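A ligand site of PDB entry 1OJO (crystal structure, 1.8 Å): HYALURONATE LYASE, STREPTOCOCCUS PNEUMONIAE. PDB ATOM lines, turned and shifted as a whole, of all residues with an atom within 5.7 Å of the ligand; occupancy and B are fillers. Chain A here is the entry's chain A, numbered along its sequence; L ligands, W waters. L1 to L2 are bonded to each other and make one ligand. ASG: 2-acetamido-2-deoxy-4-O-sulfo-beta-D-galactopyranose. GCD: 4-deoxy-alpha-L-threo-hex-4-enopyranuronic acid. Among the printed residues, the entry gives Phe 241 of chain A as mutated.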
ATOM      1  N   ARG A  76     -17.427 -13.421  -8.475  1.00  0.00           N
ATOM      2  CA  ARG A  76     -16.666 -12.731  -9.509  1.00  0.00           C
ATOM      3  C   ARG A  76     -15.401 -13.521  -9.867  1.00  0.00           C
ATOM      4  O   ARG A  76     -14.927 -13.450 -11.000  1.00  0.00           O
ATOM      5  CB  ARG A  76     -16.325 -11.300  -9.088  1.00  0.00           C
ATOM      6  CG  ARG A  76     -17.528 -10.379  -9.201  1.00  0.00           C
ATOM      7  CD  ARG A  76     -17.207  -8.916  -8.952  1.00  0.00           C
ATOM      8  NE  ARG A  76     -18.357  -8.084  -9.266  1.00  0.00           N
ATOM      9  CZ  ARG A  76     -18.420  -6.763  -9.102  1.00  0.00           C
ATOM     10  NH1 ARG A  76     -19.513  -6.107  -9.429  1.00  0.00           N
ATOM     11  NH2 ARG A  76     -17.378  -6.110  -8.602  1.00  0.00           N
ATOM     12  N   ASN A 123     -25.533  -6.061   2.890  1.00  0.00           N
ATOM     13  CA  ASN A 123     -25.983  -5.104   1.883  1.00  0.00           C
ATOM     14  C   ASN A 123     -26.826  -5.738   0.780  1.00  0.00           C
ATOM     15  O   ASN A 123     -26.416  -6.708   0.145  1.00  0.00           O
ATOM     16  CB  ASN A 123     -24.790  -4.378   1.277  1.00  0.00           C
ATOM     17  CG  ASN A 123     -25.163  -3.075   0.612  1.00  0.00           C
ATOM     18  OD1 ASN A 123     -25.958  -3.051  -0.326  1.00  0.00           O
ATOM     19  ND2 ASN A 123     -24.599  -1.973   1.108  1.00  0.00           N
ATOM     20  N   TRP A 125     -27.390  -4.683  -2.126  1.00  0.00           N
ATOM     21  CA  TRP A 125     -26.742  -4.551  -3.429  1.00  0.00           C
ATOM     22  C   TRP A 125     -26.052  -5.834  -3.897  1.00  0.00           C
ATOM     23  O   TRP A 125     -26.116  -6.188  -5.078  1.00  0.00           O
ATOM     24  CB  TRP A 125     -25.730  -3.416  -3.409  1.00  0.00           C
ATOM     25  CG  TRP A 125     -25.203  -3.067  -4.774  1.00  0.00           C
ATOM     26  CD1 TRP A 125     -25.735  -2.146  -5.644  1.00  0.00           C
ATOM     27  CD2 TRP A 125     -24.063  -3.631  -5.424  1.00  0.00           C
ATOM     28  NE1 TRP A 125     -24.987  -2.108  -6.798  1.00  0.00           N
ATOM     29  CE2 TRP A 125     -23.960  -3.006  -6.687  1.00  0.00           C
ATOM     30  CE3 TRP A 125     -23.122  -4.605  -5.067  1.00  0.00           C
ATOM     31  CZ2 TRP A 125     -22.938  -3.330  -7.594  1.00  0.00           C
ATOM     32  CZ3 TRP A 125     -22.113  -4.925  -5.972  1.00  0.00           C
ATOM     33  CH2 TRP A 125     -22.033  -4.283  -7.224  1.00  0.00           C
ATOM     34  N   ASP A 126     -25.377  -6.515  -2.972  1.00  0.00           N
ATOM     35  CA  ASP A 126     -24.677  -7.744  -3.312  1.00  0.00           C
ATOM     36  C   ASP A 126     -25.667  -8.854  -3.645  1.00  0.00           C
ATOM     37  O   ASP A 126     -25.444  -9.646  -4.570  1.00  0.00           O
ATOM     38  CB  ASP A 126     -23.795  -8.193  -2.144  1.00  0.00           C
ATOM     39  CG  ASP A 126     -22.630  -7.261  -1.909  1.00  0.00           C
ATOM     40  OD1 ASP A 126     -21.833  -7.051  -2.849  1.00  0.00           O
ATOM     41  OD2 ASP A 126     -22.496  -6.741  -0.780  1.00  0.00           O
ATOM     42  N   ARG A 133     -25.310 -10.515 -11.130  1.00  0.00           N
ATOM     43  CA  ARG A 133     -24.604 -10.194 -12.370  1.00  0.00           C
ATOM     44  C   ARG A 133     -23.443 -11.154 -12.585  1.00  0.00           C
ATOM     45  O   ARG A 133     -23.195 -11.602 -13.701  1.00  0.00           O
ATOM     46  CB  ARG A 133     -24.087  -8.751 -12.344  1.00  0.00           C
ATOM     47  CG  ARG A 133     -25.125  -7.693 -12.715  1.00  0.00           C
ATOM     48  CD  ARG A 133     -24.607  -6.314 -12.351  1.00  0.00           C
ATOM     49  NE  ARG A 133     -23.254  -6.109 -12.856  1.00  0.00           N
ATOM     50  CZ  ARG A 133     -22.438  -5.151 -12.411  1.00  0.00           C
ATOM     51  NH1 ARG A 133     -22.832  -4.313 -11.465  1.00  0.00           N
ATOM     52  NH2 ARG A 133     -21.213  -5.050 -12.917  1.00  0.00           N
ATOM     53  N   ARG A 188     -29.106  -5.696 -16.466  1.00  0.00           N
ATOM     54  CA  ARG A 188     -28.003  -6.653 -16.502  1.00  0.00           C
ATOM     55  C   ARG A 188     -28.264  -7.834 -15.574  1.00  0.00           C
ATOM     56  O   ARG A 188     -27.519  -8.816 -15.593  1.00  0.00           O
ATOM     57  CB  ARG A 188     -26.692  -5.950 -16.146  1.00  0.00           C
ATOM     58  CG  ARG A 188     -26.285  -4.909 -17.189  1.00  0.00           C
ATOM     59  CD  ARG A 188     -24.821  -4.492 -17.069  1.00  0.00           C
ATOM     60  NE  ARG A 188     -24.523  -3.736 -15.854  1.00  0.00           N
ATOM     61  CZ  ARG A 188     -23.333  -3.211 -15.588  1.00  0.00           C
ATOM     62  NH1 ARG A 188     -22.341  -3.349 -16.442  1.00  0.00           N
ATOM     63  NH2 ARG A 188     -23.139  -2.543 -14.456  1.00  0.00           N
ATOM     64  N   HIS A 232     -29.742   9.033  -5.371  1.00  0.00           N
ATOM     65  CA  HIS A 232     -29.837   8.978  -3.916  1.00  0.00           C
ATOM     66  C   HIS A 232     -30.603  10.180  -3.383  1.00  0.00           C
ATOM     67  O   HIS A 232     -30.143  10.871  -2.472  1.00  0.00           O
ATOM     68  CB  HIS A 232     -28.453   8.912  -3.290  1.00  0.00           C
ATOM     69  CG  HIS A 232     -27.803   7.565  -3.429  1.00  0.00           C
ATOM     70  ND1 HIS A 232     -26.542   7.301  -2.940  1.00  0.00           N
ATOM     71  CD2 HIS A 232     -28.244   6.416  -3.988  1.00  0.00           C
ATOM     72  CE1 HIS A 232     -26.238   6.044  -3.190  1.00  0.00           C
ATOM     73  NE2 HIS A 232     -27.257   5.480  -3.826  1.00  0.00           N
ATOM     74  N   TYR A 237     -24.634  13.277  -8.907  1.00  0.00           N
ATOM     75  CA  TYR A 237     -23.968  11.999  -9.085  1.00  0.00           C
ATOM     76  C   TYR A 237     -23.640  11.535 -10.497  1.00  0.00           C
ATOM     77  O   TYR A 237     -23.456  10.333 -10.719  1.00  0.00           O
ATOM     78  CB  TYR A 237     -24.803  10.913  -8.400  1.00  0.00           C
ATOM     79  CG  TYR A 237     -24.103  10.235  -7.237  1.00  0.00           C
ATOM     80  CD1 TYR A 237     -22.778   9.828  -7.355  1.00  0.00           C
ATOM     81  CD2 TYR A 237     -24.756   9.997  -6.027  1.00  0.00           C
ATOM     82  CE1 TYR A 237     -22.120   9.198  -6.313  1.00  0.00           C
ATOM     83  CE2 TYR A 237     -24.104   9.358  -4.966  1.00  0.00           C
ATOM     84  CZ  TYR A 237     -22.776   8.960  -5.120  1.00  0.00           C
ATOM     85  OH  TYR A 237     -22.098   8.334  -4.100  1.00  0.00           O
ATOM     86  N   ALA A 240     -20.620   8.865 -11.007  1.00  0.00           N
ATOM     87  CA  ALA A 240     -20.498   7.558 -10.362  1.00  0.00           C
ATOM     88  C   ALA A 240     -21.704   6.734 -10.771  1.00  0.00           C
ATOM     89  O   ALA A 240     -21.571   5.736 -11.468  1.00  0.00           O
ATOM     90  CB  ALA A 240     -20.421   7.714  -8.846  1.00  0.00           C
ATOM     91  N   PHE A 241     -22.896   7.147 -10.346  1.00  0.00           N
ATOM     92  CA  PHE A 241     -24.089   6.411 -10.741  1.00  0.00           C
ATOM     93  C   PHE A 241     -24.414   6.689 -12.195  1.00  0.00           C
ATOM     94  O   PHE A 241     -24.978   5.847 -12.893  1.00  0.00           O
ATOM     95  CB  PHE A 241     -25.267   6.741  -9.821  1.00  0.00           C
ATOM     96  CG  PHE A 241     -25.228   5.997  -8.525  1.00  0.00           C
ATOM     97  CD1 PHE A 241     -24.547   6.513  -7.415  1.00  0.00           C
ATOM     98  CD2 PHE A 241     -25.779   4.722  -8.425  1.00  0.00           C
ATOM     99  CE1 PHE A 241     -24.422   5.770  -6.245  1.00  0.00           C
ATOM    100  CE2 PHE A 241     -25.657   3.970  -7.261  1.00  0.00           C
ATOM    101  CZ  PHE A 241     -24.974   4.488  -6.175  1.00  0.00           C
ATOM    102  N   VAL A 244     -22.271   4.227 -14.123  1.00  0.00           N
ATOM    103  CA  VAL A 244     -22.862   2.891 -14.138  1.00  0.00           C
ATOM    104  C   VAL A 244     -23.975   2.837 -15.169  1.00  0.00           C
ATOM    105  O   VAL A 244     -24.113   1.861 -15.910  1.00  0.00           O
ATOM    106  CB  VAL A 244     -23.441   2.545 -12.737  1.00  0.00           C
ATOM    107  CG1 VAL A 244     -24.226   1.239 -12.809  1.00  0.00           C
ATOM    108  CG2 VAL A 244     -22.308   2.417 -11.740  1.00  0.00           C
ATOM    109  N   ARG A 295     -19.298   9.624  -3.269  1.00  0.00           N
ATOM    110  CA  ARG A 295     -18.381   8.912  -2.381  1.00  0.00           C
ATOM    111  C   ARG A 295     -17.301   8.093  -3.069  1.00  0.00           C
ATOM    112  O   ARG A 295     -16.391   7.598  -2.411  1.00  0.00           O
ATOM    113  CB  ARG A 295     -19.176   8.030  -1.403  1.00  0.00           C
ATOM    114  CG  ARG A 295     -19.766   6.755  -2.011  1.00  0.00           C
ATOM    115  CD  ARG A 295     -20.570   5.990  -0.949  1.00  0.00           C
ATOM    116  NE  ARG A 295     -20.740   4.574  -1.285  1.00  0.00           N
ATOM    117  CZ  ARG A 295     -21.778   4.066  -1.952  1.00  0.00           C
ATOM    118  NH1 ARG A 295     -22.770   4.846  -2.368  1.00  0.00           N
ATOM    119  NH2 ARG A 295     -21.820   2.757  -2.194  1.00  0.00           N
ATOM    120  N   SER A 296     -17.388   7.957  -4.387  1.00  0.00           N
ATOM    121  CA  SER A 296     -16.397   7.181  -5.132  1.00  0.00           C
ATOM    122  C   SER A 296     -15.013   7.810  -5.119  1.00  0.00           C
ATOM    123  O   SER A 296     -14.022   7.147  -5.462  1.00  0.00           O
ATOM    124  CB  SER A 296     -16.842   6.990  -6.588  1.00  0.00           C
ATOM    125  OG  SER A 296     -17.936   6.100  -6.643  1.00  0.00           O
ATOM    126  N   ARG A 299     -12.163   5.962  -3.236  1.00  0.00           N
ATOM    127  CA  ARG A 299     -11.701   4.649  -3.681  1.00  0.00           C
ATOM    128  C   ARG A 299     -10.376   4.815  -4.422  1.00  0.00           C
ATOM    129  O   ARG A 299     -10.302   5.517  -5.424  1.00  0.00           O
ATOM    130  CB  ARG A 299     -12.732   4.023  -4.610  1.00  0.00           C
ATOM    131  CG  ARG A 299     -14.065   3.786  -3.932  1.00  0.00           C
ATOM    132  CD  ARG A 299     -15.123   3.337  -4.915  1.00  0.00           C
ATOM    133  NE  ARG A 299     -16.424   3.237  -4.274  1.00  0.00           N
ATOM    134  CZ  ARG A 299     -17.573   3.161  -4.924  1.00  0.00           C
ATOM    135  NH1 ARG A 299     -17.592   3.182  -6.258  1.00  0.00           N
ATOM    136  NH2 ARG A 299     -18.715   3.083  -4.260  1.00  0.00           N
ATOM    137  N   SER A 302     -10.203   4.091  -8.167  1.00  0.00           N
ATOM    138  CA  SER A 302     -11.135   4.848  -8.993  1.00  0.00           C
ATOM    139  C   SER A 302     -10.881   6.345  -9.025  1.00  0.00           C
ATOM    140  O   SER A 302     -11.824   7.135  -8.936  1.00  0.00           O
ATOM    141  CB  SER A 302     -12.579   4.598  -8.508  1.00  0.00           C
ATOM    142  OG  SER A 302     -12.896   3.215  -8.562  1.00  0.00           O
ATOM    143  N   GLU A 310     -14.819   4.743 -17.609  1.00  0.00           N
ATOM    144  CA  GLU A 310     -16.125   4.097 -17.557  1.00  0.00           C
ATOM    145  C   GLU A 310     -17.067   4.842 -18.475  1.00  0.00           C
ATOM    146  O   GLU A 310     -17.883   4.248 -19.182  1.00  0.00           O
ATOM    147  CB  GLU A 310     -16.711   4.131 -16.138  1.00  0.00           C
ATOM    148  CG  GLU A 310     -16.008   3.272 -15.118  1.00  0.00           C
ATOM    149  CD  GLU A 310     -16.837   3.150 -13.851  1.00  0.00           C
ATOM    150  OE1 GLU A 310     -17.280   4.183 -13.326  1.00  0.00           O
ATOM    151  OE2 GLU A 310     -17.033   2.014 -13.382  1.00  0.00           O
ATOM    152  N   ASN A 413     -21.907   3.409   3.527  1.00  0.00           N
ATOM    153  CA  ASN A 413     -21.215   2.153   3.296  1.00  0.00           C
ATOM    154  C   ASN A 413     -19.765   2.309   3.728  1.00  0.00           C
ATOM    155  O   ASN A 413     -18.862   1.674   3.192  1.00  0.00           O
ATOM    156  CB  ASN A 413     -21.288   1.723   1.822  1.00  0.00           C
ATOM    157  CG  ASN A 413     -22.691   1.286   1.427  1.00  0.00           C
ATOM    158  OD1 ASN A 413     -23.580   1.163   2.264  1.00  0.00           O
ATOM    159  ND2 ASN A 413     -22.892   1.048   0.135  1.00  0.00           N
ATOM    160  N   GLU A 415     -17.803   4.781   3.285  1.00  0.00           N
ATOM    161  CA  GLU A 415     -16.985   5.459   2.285  1.00  0.00           C
ATOM    162  C   GLU A 415     -17.121   6.979   2.359  1.00  0.00           C
ATOM    163  O   GLU A 415     -18.204   7.496   2.658  1.00  0.00           O
ATOM    164  CB  GLU A 415     -17.374   4.995   0.889  1.00  0.00           C
ATOM    165  CG  GLU A 415     -17.248   3.501   0.663  1.00  0.00           C
ATOM    166  CD  GLU A 415     -17.385   3.124  -0.803  1.00  0.00           C
ATOM    167  OE1 GLU A 415     -18.505   3.163  -1.335  1.00  0.00           O
ATOM    168  OE2 GLU A 415     -16.352   2.805  -1.429  1.00  0.00           O
HETATM  169  C1  ASG L   1     -22.853   0.671  -4.978  1.00  0.00           C
HETATM  170  C2  ASG L   1     -21.649   1.206  -5.776  1.00  0.00           C
HETATM  171  C3  ASG L   1     -20.871   0.030  -6.359  1.00  0.00           C
HETATM  172  C4  ASG L   1     -20.364  -0.965  -5.216  1.00  0.00           C
HETATM  173  C5  ASG L   1     -21.574  -1.464  -4.429  1.00  0.00           C
HETATM  174  C6  ASG L   1     -21.131  -2.391  -3.301  1.00  0.00           C
HETATM  175  C7  ASG L   1     -21.546   3.428  -6.990  1.00  0.00           C
HETATM  176  C8  ASG L   1     -22.040   4.175  -8.200  1.00  0.00           C
HETATM  177  O1  ASG L   1     -23.571   1.759  -4.426  1.00  0.00           O
HETATM  178  N2  ASG L   1     -22.073   2.108  -6.919  1.00  0.00           N
HETATM  179  O3  ASG L   1     -19.793   0.610  -7.110  1.00  0.00           O
HETATM  180  O4  ASG L   1     -19.403  -0.279  -4.484  1.00  0.00           O
HETATM  181  O5  ASG L   1     -22.355  -0.259  -3.869  1.00  0.00           O
HETATM  182  O6  ASG L   1     -22.223  -2.734  -2.406  1.00  0.00           O
HETATM  183  O7  ASG L   1     -20.747   3.927  -6.143  1.00  0.00           O
HETATM  184  OSA ASG L   1     -18.077  -2.244  -3.994  1.00  0.00           O
HETATM  185  OSB ASG L   1     -17.201  -0.061  -3.471  1.00  0.00           O
HETATM  186  OSC ASG L   1     -17.396  -0.762  -5.770  1.00  0.00           O
HETATM  187  S   ASG L   1     -18.017  -0.840  -4.432  1.00  0.00           S
HETATM  188  C1  GCD L   2     -19.688   0.470  -8.489  1.00  0.00           C
HETATM  189  C2  GCD L   2     -18.488   1.207  -8.979  1.00  0.00           C
HETATM  190  C3  GCD L   2     -18.423   0.979 -10.533  1.00  0.00           C
HETATM  191  C4  GCD L   2     -18.761  -0.415 -11.133  1.00  0.00           C
HETATM  192  C5  GCD L   2     -19.197  -1.382 -10.261  1.00  0.00           C
HETATM  193  C6  GCD L   2     -19.565  -2.783 -10.646  1.00  0.00           C
HETATM  194  O2  GCD L   2     -18.693   2.642  -8.741  1.00  0.00           O
HETATM  195  O3  GCD L   2     -17.179   1.632 -10.866  1.00  0.00           O
HETATM  196  O5  GCD L   2     -19.350  -1.018  -8.770  1.00  0.00           O
HETATM  197  O6A GCD L   2     -19.582  -3.556  -9.621  1.00  0.00           O
HETATM  198  O6B GCD L   2     -19.815  -3.026 -11.874  1.00  0.00           O
HETATM  199  O   HOH W   1     -15.896   4.749 -10.682  1.00  0.00           O
HETATM  200  O   HOH W   2     -20.229   6.457  -5.540  1.00  0.00           O
HETATM  201  O   HOH W   3     -18.986   4.401 -11.048  1.00  0.00           O
HETATM  202  O   HOH W   4     -18.789  -3.648  -1.298  1.00  0.00           O
HETATM  203  O   HOH W   5     -26.623   1.093  -5.646  1.00  0.00           O
HETATM  204  O   HOH W   6     -24.402  -0.751  -1.647  1.00  0.00           O
HETATM  205  O   HOH W   7     -20.073   0.647  -1.686  1.00  0.00           O
HETATM  206  O   HOH W   8     -18.092  -2.989 -13.801  1.00  0.00           O
HETATM  207  O   HOH W   9     -21.283  -4.309  -0.206  1.00  0.00           O
HETATM  208  O   HOH W  10     -18.510  -5.133  -5.485  1.00  0.00           O
HETATM  209  O   HOH W  11     -21.081  -1.057 -13.254  1.00  0.00           O
HETATM  210  O   HOH W  12     -23.470   0.599  -8.757  1.00  0.00           O
HETATM  211  O   HOH W  13     -15.638   2.996  -8.338  1.00  0.00           O
HETATM  212  O   HOH W  14     -25.864   0.901  -3.225  1.00  0.00           O
HETATM  213  O   HOH W  15     -18.243  -3.336  -7.346  1.00  0.00           O
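The side-chain hydroxyl (OG) of Ser 296 sits at hydrogen-bond distance from the guanidinium group (NH1) of Arg 299 (3.0 Å). NE of Arg 299 is in salt-bridge range of OE2 of Glu 415 (2.9 Å). The guanidinium group of Arg 295 lies within salt-bridge range of the side-chain carboxylate of Glu 415, 2.6 Å away. The guanidinium group of Arg 295 sits close to the side-chain amide nitrogen of Asn 413 (3.1 Å). The side-chain hydroxyl of Tyr 237 lies within hydrogen-bond range of the backbone NH of Arg 295 (3.2 Å). The backbone NH of Trp 125 is in hydrogen-bond range of the side-chain amide oxygen of Asn 123.
Water W2 lies within hydrogen-bond range of OG of Ser 296 (2.6 Å), O7 of ASG L1 (2.7 Å) and OH of Tyr 237 (3.0 Å). Water W9 lies within hydrogen-bond range of OD2 of Asp 126 (2.8 Å) and O6 of ASG L1 (2.9 Å). Water W3 lies within hydrogen-bond range of OE1 of Glu 310 (2.9 Å), O2 of GCD L2 (2.9 Å) and O of Ala 240 (2.9 Å). Water W13 lies within hydrogen-bond range of the side-chain hydroxyl (OG) of Ser 302 (2.8 Å), the guanidinium group (NH1) of Arg 299 (2.9 Å) and an oxygen (O2) of GCD L2 (3.1 Å). Water W10 bridges OSA of ASG L1 (3.3 Å) and NH2 of Arg 76 (3.5 Å). Water W1 bridges OE1 of Glu 310 (3.0 Å) and O3 of GCD L2 (3.4 Å).
The side-chain carboxylate (OE2) of Glu 310 lies within hydrogen-bond range of an oxygen (O3) of GCD L2, 2.5 Å away. The guanidinium group of Arg 76 lies within salt-bridge range of an oxygen (O6A) of GCD L2. An oxygen (O6B) of GCD L2 lies within salt-bridge range of the guanidinium group (NH2) of Arg 133, at 2.7 Å. OSB of ASG L1 is in salt-bridge range of NE of Arg 299 (3.5 Å). An oxygen (O1) of ASG L1 lies within hydrogen-bond range of the guanidinium group (NH2) of Arg 295, 3.0 Å away.
Trp 125 touches the ligand. C of Ala 240 touches C8 of ASG L1, 3.6 Å away. CE1 of Phe 241 touches C8 of ASG L1, at 3.5 Å. CG2 of Val 244 touches C8 of ASG L1, 3.96 Å away. OG of Ser 296 touches O7 of ASG L1, 3.6 Å away. OE2 of Glu 415 touches OSB of ASG L1, at 3.6 Å. Hydrophobic or aromatic side chains within 4 Å of the ligand: Trp 125, Ala 240, Phe 241 and Val 244. 11 residues have an atom within 4 Å of the ligand: Arg 76, Trp 125, Arg 133, Ala 240, Phe 241, Val 244, Arg 295, Ser 296, Arg 299, Glu 310 and Glu 415.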
